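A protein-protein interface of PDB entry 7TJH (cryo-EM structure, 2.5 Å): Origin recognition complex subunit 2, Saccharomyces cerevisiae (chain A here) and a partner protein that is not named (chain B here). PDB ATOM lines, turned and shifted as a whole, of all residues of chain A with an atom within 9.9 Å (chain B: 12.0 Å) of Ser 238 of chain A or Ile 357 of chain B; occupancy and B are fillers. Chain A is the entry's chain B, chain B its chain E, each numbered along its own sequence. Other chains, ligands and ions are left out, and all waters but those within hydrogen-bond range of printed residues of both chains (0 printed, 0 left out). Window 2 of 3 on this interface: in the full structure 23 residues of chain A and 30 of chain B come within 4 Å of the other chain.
The backbone NH of Lys 353 of chain B lies within hydrogen-bond range of the side-chain carboxylate of Glu 244 of chain A.
The side-chain hydroxyl of Ser 351 of chain B lies close to the side-chain carboxylate of Glu 244 of chain A (3.3 Å).
NH2 of Arg 355 of chain B lies within salt-bridge range of OD1 of Asp 248 of chain A (2.9 Å).
The backbone NH (N) of Arg 352 of chain B sits at hydrogen-bond distance from the side-chain carboxylate (OE2) of Glu 244 of chain A (2.9 Å).
The backbone carbonyl oxygen of Ile 357 of chain B sits at hydrogen-bond distance from the side-chain hydroxyl of Ser 238 of chain A (3.2 Å).
The side-chain carboxylate of Asp 248 of chain A sits at hydrogen-bond distance from the backbone NH of Ser 238 of chain A, at 2.9 Å.
The side-chain hydroxyl (OG) of Ser 237 of chain A lies within hydrogen-bond range of the backbone carbonyl oxygen (O) of Phe 239 of chain A (3.2 Å).
Among the printed residues, merely in contact across the chains: Ser 237 of chain A with Ile 357 of chain B, Ser 238 of chain A with Arg 355 of chain B, Phe 239 of chain A with Lys 353 of chain B, Phe 239 of chain A with Thr 354 of chain B, Phe 239 of chain A with Arg 355 of chain B and Phe 247 of chain A with Ala 347 of chain B.
Ser 238 of chain A touches just these residues of chain B: Arg 355 (3.4 Å) and Ile 357 (3.2 Å).
Ile 357 of chain B touches just these residues of chain A: Ser 237 (3.4 Å) and Ser 238 (3.2 Å).
No residue of chain B comes within 4 Å of Ala 236 of chain A.
No residue of chain B comes within 4 Å of Gly 245 of chain A.
Of chain A, only Ser 238 (3.4 Å), Phe 239 (3.4 Å) and Asp 248 (2.9 Å) come within 4 Å of Arg 355 of chain B.
No residue of chain A comes within 4 Å of Ile 356 of chain B.
Printed residues of chain A within 4 Å of Arg 352 of chain B: Glu 244 (2.9 Å).
Of the printed residues of chain B, Phe 247 of chain A touches Ala 347 (3.96 Å).
Arg 360 of chain B touches none of the printed residues of chain A.
Gln 249 of chain A touches none of the printed residues of chain B.
The nearest residue of chain B that does not touch Ser 238 of chain A is Ile 356 of chain B (4.2 Å).
The nearest residue of chain A that does not touch Ile 357 of chain B is Phe 239 of chain A (5.9 Å).
Among the printed residues, 11 pairs touch across the chains.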
ATOM      1  N   SER A 235     -28.364  34.218 -15.912  1.00  0.00           N
ATOM      2  CA  SER A 235     -27.970  32.823 -16.045  1.00  0.00           C
ATOM      3  C   SER A 235     -26.461  32.675 -15.921  1.00  0.00           C
ATOM      4  O   SER A 235     -25.705  33.481 -16.461  1.00  0.00           O
ATOM      5  CB  SER A 235     -28.440  32.250 -17.389  1.00  0.00           C
ATOM      6  OG  SER A 235     -27.960  30.931 -17.580  1.00  0.00           O
ATOM      7  N   ALA A 236     -26.026  31.634 -15.209  1.00  0.00           N
ATOM      8  CA  ALA A 236     -24.608  31.285 -15.128  1.00  0.00           C
ATOM      9  C   ALA A 236     -24.232  30.498 -16.384  1.00  0.00           C
ATOM     10  O   ALA A 236     -24.048  29.279 -16.378  1.00  0.00           O
ATOM     11  CB  ALA A 236     -24.316  30.500 -13.858  1.00  0.00           C
ATOM     12  N   SER A 237     -24.126  31.235 -17.485  1.00  0.00           N
ATOM     13  CA  SER A 237     -23.941  30.664 -18.805  1.00  0.00           C
ATOM     14  C   SER A 237     -22.849  31.428 -19.535  1.00  0.00           C
ATOM     15  O   SER A 237     -22.507  32.558 -19.180  1.00  0.00           O
ATOM     16  CB  SER A 237     -25.244  30.704 -19.617  1.00  0.00           C
ATOM     17  OG  SER A 237     -25.195  29.814 -20.715  1.00  0.00           O
ATOM     18  N   SER A 238     -22.298  30.788 -20.561  1.00  0.00           N
ATOM     19  CA  SER A 238     -21.302  31.417 -21.415  1.00  0.00           C
ATOM     20  C   SER A 238     -21.883  31.943 -22.714  1.00  0.00           C
ATOM     21  O   SER A 238     -21.334  32.890 -23.287  1.00  0.00           O
ATOM     22  CB  SER A 238     -20.175  30.429 -21.732  1.00  0.00           C
ATOM     23  OG  SER A 238     -19.192  31.025 -22.556  1.00  0.00           O
ATOM     24  N   PHE A 239     -22.975  31.357 -23.193  1.00  0.00           N
ATOM     25  CA  PHE A 239     -23.612  31.771 -24.431  1.00  0.00           C
ATOM     26  C   PHE A 239     -25.047  32.192 -24.154  1.00  0.00           C
ATOM     27  O   PHE A 239     -25.690  31.690 -23.229  1.00  0.00           O
ATOM     28  CB  PHE A 239     -23.598  30.646 -25.465  1.00  0.00           C
ATOM     29  CG  PHE A 239     -22.284  29.942 -25.572  1.00  0.00           C
ATOM     30  CD1 PHE A 239     -21.144  30.629 -25.955  1.00  0.00           C
ATOM     31  CD2 PHE A 239     -22.187  28.588 -25.285  1.00  0.00           C
ATOM     32  CE1 PHE A 239     -19.931  29.980 -26.049  1.00  0.00           C
ATOM     33  CE2 PHE A 239     -20.979  27.933 -25.377  1.00  0.00           C
ATOM     34  CZ  PHE A 239     -19.851  28.627 -25.764  1.00  0.00           C
ATOM     35  N   LEU A 240     -25.541  33.128 -24.960  1.00  0.00           N
ATOM     36  CA  LEU A 240     -26.942  33.520 -24.907  1.00  0.00           C
ATOM     37  C   LEU A 240     -27.668  33.194 -26.199  1.00  0.00           C
ATOM     38  O   LEU A 240     -28.706  32.524 -26.175  1.00  0.00           O
ATOM     39  CB  LEU A 240     -27.075  35.021 -24.614  1.00  0.00           C
ATOM     40  CG  LEU A 240     -26.384  35.578 -23.370  1.00  0.00           C
ATOM     41  CD1 LEU A 240     -25.789  36.925 -23.700  1.00  0.00           C
ATOM     42  CD2 LEU A 240     -27.337  35.684 -22.203  1.00  0.00           C
ATOM     43  N   ASP A 241     -27.136  33.639 -27.327  1.00  0.00           N
ATOM     44  CA  ASP A 241     -27.784  33.472 -28.613  1.00  0.00           C
ATOM     45  C   ASP A 241     -27.423  32.123 -29.221  1.00  0.00           C
ATOM     46  O   ASP A 241     -26.624  31.365 -28.673  1.00  0.00           O
ATOM     47  CB  ASP A 241     -27.388  34.609 -29.548  1.00  0.00           C
ATOM     48  CG  ASP A 241     -28.088  35.901 -29.209  1.00  0.00           C
ATOM     49  OD1 ASP A 241     -28.953  35.890 -28.309  1.00  0.00           O
ATOM     50  OD2 ASP A 241     -27.765  36.931 -29.831  1.00  0.00           O
ATOM     51  N   THR A 242     -28.077  31.822 -30.350  1.00  0.00           N
ATOM     52  CA  THR A 242     -27.908  30.665 -31.235  1.00  0.00           C
ATOM     53  C   THR A 242     -28.046  29.313 -30.516  1.00  0.00           C
ATOM     54  O   THR A 242     -28.472  29.252 -29.351  1.00  0.00           O
ATOM     55  CB  THR A 242     -26.597  30.804 -32.061  1.00  0.00           C
ATOM     56  OG1 THR A 242     -26.729  30.081 -33.288  1.00  0.00           O
ATOM     57  CG2 THR A 242     -25.296  30.343 -31.359  1.00  0.00           C
ATOM     58  N   GLU A 244     -25.788  27.427 -29.485  1.00  0.00           N
ATOM     59  CA  GLU A 244     -24.880  27.432 -28.342  1.00  0.00           C
ATOM     60  C   GLU A 244     -25.576  27.926 -27.080  1.00  0.00           C
ATOM     61  O   GLU A 244     -25.465  27.304 -26.021  1.00  0.00           O
ATOM     62  CB  GLU A 244     -23.656  28.292 -28.664  1.00  0.00           C
ATOM     63  CG  GLU A 244     -22.905  27.875 -29.934  1.00  0.00           C
ATOM     64  CD  GLU A 244     -21.965  26.685 -29.757  1.00  0.00           C
ATOM     65  OE1 GLU A 244     -22.101  25.916 -28.787  1.00  0.00           O
ATOM     66  OE2 GLU A 244     -21.033  26.553 -30.578  1.00  0.00           O
ATOM     67  N   GLY A 245     -26.315  29.032 -27.183  1.00  0.00           N
ATOM     68  CA  GLY A 245     -27.078  29.513 -26.041  1.00  0.00           C
ATOM     69  C   GLY A 245     -28.219  28.590 -25.664  1.00  0.00           C
ATOM     70  O   GLY A 245     -28.533  28.439 -24.477  1.00  0.00           O
ATOM     71  N   TYR A 246     -28.848  27.960 -26.667  1.00  0.00           N
ATOM     72  CA  TYR A 246     -29.904  26.982 -26.401  1.00  0.00           C
ATOM     73  C   TYR A 246     -29.381  25.800 -25.592  1.00  0.00           C
ATOM     74  O   TYR A 246     -30.004  25.384 -24.608  1.00  0.00           O
ATOM     75  CB  TYR A 246     -30.517  26.488 -27.714  1.00  0.00           C
ATOM     76  CG  TYR A 246     -31.644  25.494 -27.515  1.00  0.00           C
ATOM     77  CD1 TYR A 246     -32.923  25.926 -27.184  1.00  0.00           C
ATOM     78  CD2 TYR A 246     -31.430  24.122 -27.658  1.00  0.00           C
ATOM     79  CE1 TYR A 246     -33.956  25.027 -26.999  1.00  0.00           C
ATOM     80  CE2 TYR A 246     -32.455  23.215 -27.468  1.00  0.00           C
ATOM     81  CZ  TYR A 246     -33.717  23.674 -27.142  1.00  0.00           C
ATOM     82  OH  TYR A 246     -34.739  22.780 -26.953  1.00  0.00           O
ATOM     83  N   PHE A 247     -28.237  25.248 -25.986  1.00  0.00           N
ATOM     84  CA  PHE A 247     -27.695  24.104 -25.264  1.00  0.00           C
ATOM     85  C   PHE A 247     -27.057  24.506 -23.940  1.00  0.00           C
ATOM     86  O   PHE A 247     -27.112  23.735 -22.977  1.00  0.00           O
ATOM     87  CB  PHE A 247     -26.687  23.357 -26.138  1.00  0.00           C
ATOM     88  CG  PHE A 247     -27.299  22.715 -27.349  1.00  0.00           C
ATOM     89  CD1 PHE A 247     -28.538  22.100 -27.268  1.00  0.00           C
ATOM     90  CD2 PHE A 247     -26.637  22.722 -28.565  1.00  0.00           C
ATOM     91  CE1 PHE A 247     -29.110  21.510 -28.382  1.00  0.00           C
ATOM     92  CE2 PHE A 247     -27.203  22.139 -29.684  1.00  0.00           C
ATOM     93  CZ  PHE A 247     -28.440  21.528 -29.591  1.00  0.00           C
ATOM     94  N   ASP A 248     -26.463  25.700 -23.860  1.00  0.00           N
ATOM     95  CA  ASP A 248     -25.771  26.098 -22.642  1.00  0.00           C
ATOM     96  C   ASP A 248     -26.730  26.545 -21.550  1.00  0.00           C
ATOM     97  O   ASP A 248     -26.427  26.373 -20.365  1.00  0.00           O
ATOM     98  CB  ASP A 248     -24.765  27.209 -22.952  1.00  0.00           C
ATOM     99  CG  ASP A 248     -23.628  27.261 -21.952  1.00  0.00           C
ATOM    100  OD1 ASP A 248     -22.837  26.295 -21.905  1.00  0.00           O
ATOM    101  OD2 ASP A 248     -23.513  28.268 -21.223  1.00  0.00           O
ATOM    102  N   GLN A 249     -27.881  27.113 -21.907  1.00  0.00           N
ATOM    103  CA  GLN A 249     -28.807  27.581 -20.885  1.00  0.00           C
ATOM    104  C   GLN A 249     -29.771  26.502 -20.407  1.00  0.00           C
ATOM    105  O   GLN A 249     -30.487  26.728 -19.426  1.00  0.00           O
ATOM    106  CB  GLN A 249     -29.588  28.794 -21.397  1.00  0.00           C
ATOM    107  CG  GLN A 249     -28.830  30.101 -21.238  1.00  0.00           C
ATOM    108  CD  GLN A 249     -29.583  31.293 -21.789  1.00  0.00           C
ATOM    109  OE1 GLN A 249     -30.159  31.229 -22.873  1.00  0.00           O
ATOM    110  NE2 GLN A 249     -29.582  32.392 -21.041  1.00  0.00           N
ATOM    111  N   ARG A 250     -29.812  25.350 -21.066  1.00  0.00           N
ATOM    112  CA  ARG A 250     -30.629  24.224 -20.617  1.00  0.00           C
ATOM    113  C   ARG A 250     -29.777  23.190 -19.882  1.00  0.00           C
ATOM    114  O   ARG A 250     -29.610  22.053 -20.318  1.00  0.00           O
ATOM    115  CB  ARG A 250     -31.361  23.599 -21.797  1.00  0.00           C
ATOM    116  CG  ARG A 250     -32.345  24.534 -22.459  1.00  0.00           C
ATOM    117  CD  ARG A 250     -32.872  23.946 -23.743  1.00  0.00           C
ATOM    118  NE  ARG A 250     -33.703  22.774 -23.505  1.00  0.00           N
ATOM    119  CZ  ARG A 250     -35.028  22.788 -23.491  1.00  0.00           C
ATOM    120  NH1 ARG A 250     -35.709  23.901 -23.696  1.00  0.00           N
ATOM    121  NH2 ARG A 250     -35.685  21.656 -23.259  1.00  0.00           N
ATOM    122  N   LYS A 251     -29.234  23.603 -18.745  1.00  0.00           N
ATOM    123  CA  LYS A 251     -28.451  22.720 -17.897  1.00  0.00           C
ATOM    124  C   LYS A 251     -29.300  22.223 -16.732  1.00  0.00           C
ATOM    125  O   LYS A 251     -30.292  22.845 -16.344  1.00  0.00           O
ATOM    126  CB  LYS A 251     -27.200  23.436 -17.383  1.00  0.00           C
ATOM    127  CG  LYS A 251     -26.058  23.478 -18.402  1.00  0.00           C
ATOM    128  CD  LYS A 251     -24.768  24.162 -17.910  1.00  0.00           C
ATOM    129  CE  LYS A 251     -24.826  24.680 -16.473  1.00  0.00           C
ATOM    130  NZ  LYS A 251     -23.495  25.147 -15.999  1.00  0.00           N
ATOM    131  N   ALA B 347     -25.002  19.158 -26.193  1.00  0.00           N
ATOM    132  CA  ALA B 347     -23.879  20.071 -26.002  1.00  0.00           C
ATOM    133  C   ALA B 347     -22.526  19.367 -26.050  1.00  0.00           C
ATOM    134  O   ALA B 347     -21.513  20.017 -26.318  1.00  0.00           O
ATOM    135  CB  ALA B 347     -24.027  20.809 -24.673  1.00  0.00           C
ATOM    136  N   SER B 351     -21.476  21.614 -29.611  1.00  0.00           N
ATOM    137  CA  SER B 351     -20.952  22.886 -29.129  1.00  0.00           C
ATOM    138  C   SER B 351     -19.515  23.102 -29.594  1.00  0.00           C
ATOM    139  O   SER B 351     -18.646  22.253 -29.379  1.00  0.00           O
ATOM    140  CB  SER B 351     -21.033  22.959 -27.605  1.00  0.00           C
ATOM    141  OG  SER B 351     -20.149  23.935 -27.089  1.00  0.00           O
ATOM    142  N   ARG B 352     -19.272  24.248 -30.238  1.00  0.00           N
ATOM    143  CA  ARG B 352     -17.960  24.536 -30.805  1.00  0.00           C
ATOM    144  C   ARG B 352     -17.536  25.994 -30.660  1.00  0.00           C
ATOM    145  O   ARG B 352     -16.560  26.400 -31.303  1.00  0.00           O
ATOM    146  CB  ARG B 352     -17.936  24.138 -32.282  1.00  0.00           C
ATOM    147  CG  ARG B 352     -18.937  24.898 -33.132  1.00  0.00           C
ATOM    148  CD  ARG B 352     -19.513  24.016 -34.218  1.00  0.00           C
ATOM    149  NE  ARG B 352     -20.096  24.799 -35.299  1.00  0.00           N
ATOM    150  CZ  ARG B 352     -21.090  24.384 -36.071  1.00  0.00           C
ATOM    151  NH1 ARG B 352     -21.643  23.194 -35.903  1.00  0.00           N
ATOM    152  NH2 ARG B 352     -21.541  25.181 -37.034  1.00  0.00           N
ATOM    153  N   LYS B 353     -18.218  26.789 -29.843  1.00  0.00           N
ATOM    154  CA  LYS B 353     -17.930  28.213 -29.750  1.00  0.00           C
ATOM    155  C   LYS B 353     -16.862  28.496 -28.698  1.00  0.00           C
ATOM    156  O   LYS B 353     -16.648  27.720 -27.764  1.00  0.00           O
ATOM    157  CB  LYS B 353     -19.198  29.002 -29.425  1.00  0.00           C
ATOM    158  CG  LYS B 353     -19.379  30.254 -30.260  1.00  0.00           C
ATOM    159  CD  LYS B 353     -20.374  31.211 -29.623  1.00  0.00           C
ATOM    160  CE  LYS B 353     -20.586  32.434 -30.491  1.00  0.00           C
ATOM    161  NZ  LYS B 353     -21.430  33.455 -29.818  1.00  0.00           N
ATOM    162  N   THR B 354     -16.194  29.635 -28.863  1.00  0.00           N
ATOM    163  CA  THR B 354     -15.167  30.067 -27.927  1.00  0.00           C
ATOM    164  C   THR B 354     -15.816  30.764 -26.739  1.00  0.00           C
ATOM    165  O   THR B 354     -16.608  31.696 -26.911  1.00  0.00           O
ATOM    166  CB  THR B 354     -14.176  31.003 -28.621  1.00  0.00           C
ATOM    167  OG1 THR B 354     -13.557  30.317 -29.718  1.00  0.00           O
ATOM    168  CG2 THR B 354     -13.099  31.465 -27.654  1.00  0.00           C
ATOM    169  N   ARG B 355     -15.477  30.315 -25.534  1.00  0.00           N
ATOM    170  CA  ARG B 355     -16.110  30.803 -24.310  1.00  0.00           C
ATOM    171  C   ARG B 355     -15.334  31.997 -23.768  1.00  0.00           C
ATOM    172  O   ARG B 355     -14.252  31.845 -23.195  1.00  0.00           O
ATOM    173  CB  ARG B 355     -16.206  29.685 -23.280  1.00  0.00           C
ATOM    174  CG  ARG B 355     -16.843  28.421 -23.810  1.00  0.00           C
ATOM    175  CD  ARG B 355     -17.286  27.502 -22.686  1.00  0.00           C
ATOM    176  NE  ARG B 355     -18.299  26.557 -23.139  1.00  0.00           N
ATOM    177  CZ  ARG B 355     -19.478  26.389 -22.554  1.00  0.00           C
ATOM    178  NH1 ARG B 355     -19.799  27.039 -21.449  1.00  0.00           N
ATOM    179  NH2 ARG B 355     -20.355  25.549 -23.094  1.00  0.00           N
ATOM    180  N   ILE B 356     -15.891  33.194 -23.969  1.00  0.00           N
ATOM    181  CA  ILE B 356     -15.411  34.382 -23.268  1.00  0.00           C
ATOM    182  C   ILE B 356     -15.635  34.227 -21.771  1.00  0.00           C
ATOM    183  O   ILE B 356     -14.754  34.526 -20.954  1.00  0.00           O
ATOM    184  CB  ILE B 356     -16.118  35.638 -23.820  1.00  0.00           C
ATOM    185  CG1 ILE B 356     -15.782  35.848 -25.299  1.00  0.00           C
ATOM    186  CG2 ILE B 356     -15.761  36.876 -23.010  1.00  0.00           C
ATOM    187  CD1 ILE B 356     -14.310  35.808 -25.611  1.00  0.00           C
ATOM    188  N   ILE B 357     -16.799  33.735 -21.397  1.00  0.00           N
ATOM    189  CA  ILE B 357     -17.169  33.503 -20.009  1.00  0.00           C
ATOM    190  C   ILE B 357     -16.752  32.094 -19.614  1.00  0.00           C
ATOM    191  O   ILE B 357     -16.878  31.154 -20.408  1.00  0.00           O
ATOM    192  CB  ILE B 357     -18.679  33.751 -19.813  1.00  0.00           C
ATOM    193  CG1 ILE B 357     -18.956  35.250 -19.896  1.00  0.00           C
ATOM    194  CG2 ILE B 357     -19.209  33.182 -18.503  1.00  0.00           C
ATOM    195  CD1 ILE B 357     -19.554  35.674 -21.189  1.00  0.00           C
ATOM    196  N   GLN B 358     -16.180  31.971 -18.410  1.00  0.00           N
ATOM    197  CA  GLN B 358     -15.839  30.682 -17.818  1.00  0.00           C
ATOM    198  C   GLN B 358     -17.060  29.776 -17.733  1.00  0.00           C
ATOM    199  O   GLN B 358     -18.037  30.094 -17.048  1.00  0.00           O
ATOM    200  CB  GLN B 358     -15.246  30.896 -16.427  1.00  0.00           C
ATOM    201  CG  GLN B 358     -13.777  31.263 -16.424  1.00  0.00           C
ATOM    202  CD  GLN B 358     -13.301  31.742 -15.066  1.00  0.00           C
ATOM    203  OE1 GLN B 358     -13.985  31.566 -14.059  1.00  0.00           O
ATOM    204  NE2 GLN B 358     -12.119  32.343 -15.033  1.00  0.00           N
ATOM    205  N   GLY B 359     -17.004  28.656 -18.443  1.00  0.00           N
ATOM    206  CA  GLY B 359     -18.099  27.710 -18.458  1.00  0.00           C
ATOM    207  C   GLY B 359     -17.650  26.316 -18.838  1.00  0.00           C
ATOM    208  O   GLY B 359     -16.788  26.152 -19.705  1.00  0.00           O
ATOM    209  N   ARG B 360     -18.224  25.304 -18.198  1.00  0.00           N
ATOM    210  CA  ARG B 360     -17.853  23.916 -18.428  1.00  0.00           C
ATOM    211  C   ARG B 360     -18.860  23.283 -19.386  1.00  0.00           C
ATOM    212  O   ARG B 360     -20.069  23.326 -19.144  1.00  0.00           O
ATOM    213  CB  ARG B 360     -17.778  23.173 -17.096  1.00  0.00           C
ATOM    214  CG  ARG B 360     -17.309  21.744 -17.176  1.00  0.00           C
ATOM    215  CD  ARG B 360     -17.322  21.129 -15.792  1.00  0.00           C
ATOM    216  NE  ARG B 360     -16.356  21.764 -14.900  1.00  0.00           N
ATOM    217  CZ  ARG B 360     -15.069  21.443 -14.839  1.00  0.00           C
ATOM    218  NH1 ARG B 360     -14.560  20.484 -15.592  1.00  0.00           N
ATOM    219  NH2 ARG B 360     -14.277  22.098 -13.996  1.00  0.00           N
ATOM    220  N   ALA B 361     -18.315  22.782 -20.484  1.00  0.00           N
ATOM    221  CA  ALA B 361     -19.176  22.121 -21.472  1.00  0.00           C
ATOM    222  C   ALA B 361     -19.646  20.805 -20.870  1.00  0.00           C
ATOM    223  O   ALA B 361     -19.254  20.489 -19.733  1.00  0.00           O
ATOM    224  CB  ALA B 361     -18.383  21.898 -22.715  1.00  0.00           C
ATOM    225  N   ALA B 362     -20.458  20.069 -21.619  1.00  0.00           N
ATOM    226  CA  ALA B 362     -20.961  18.784 -21.109  1.00  0.00           C
ATOM    227  C   ALA B 362     -19.825  17.768 -21.148  1.00  0.00           C
ATOM    228  O   ALA B 362     -18.952  17.899 -22.012  1.00  0.00           O
ATOM    229  CB  ALA B 362     -22.134  18.353 -21.936  1.00  0.00           C
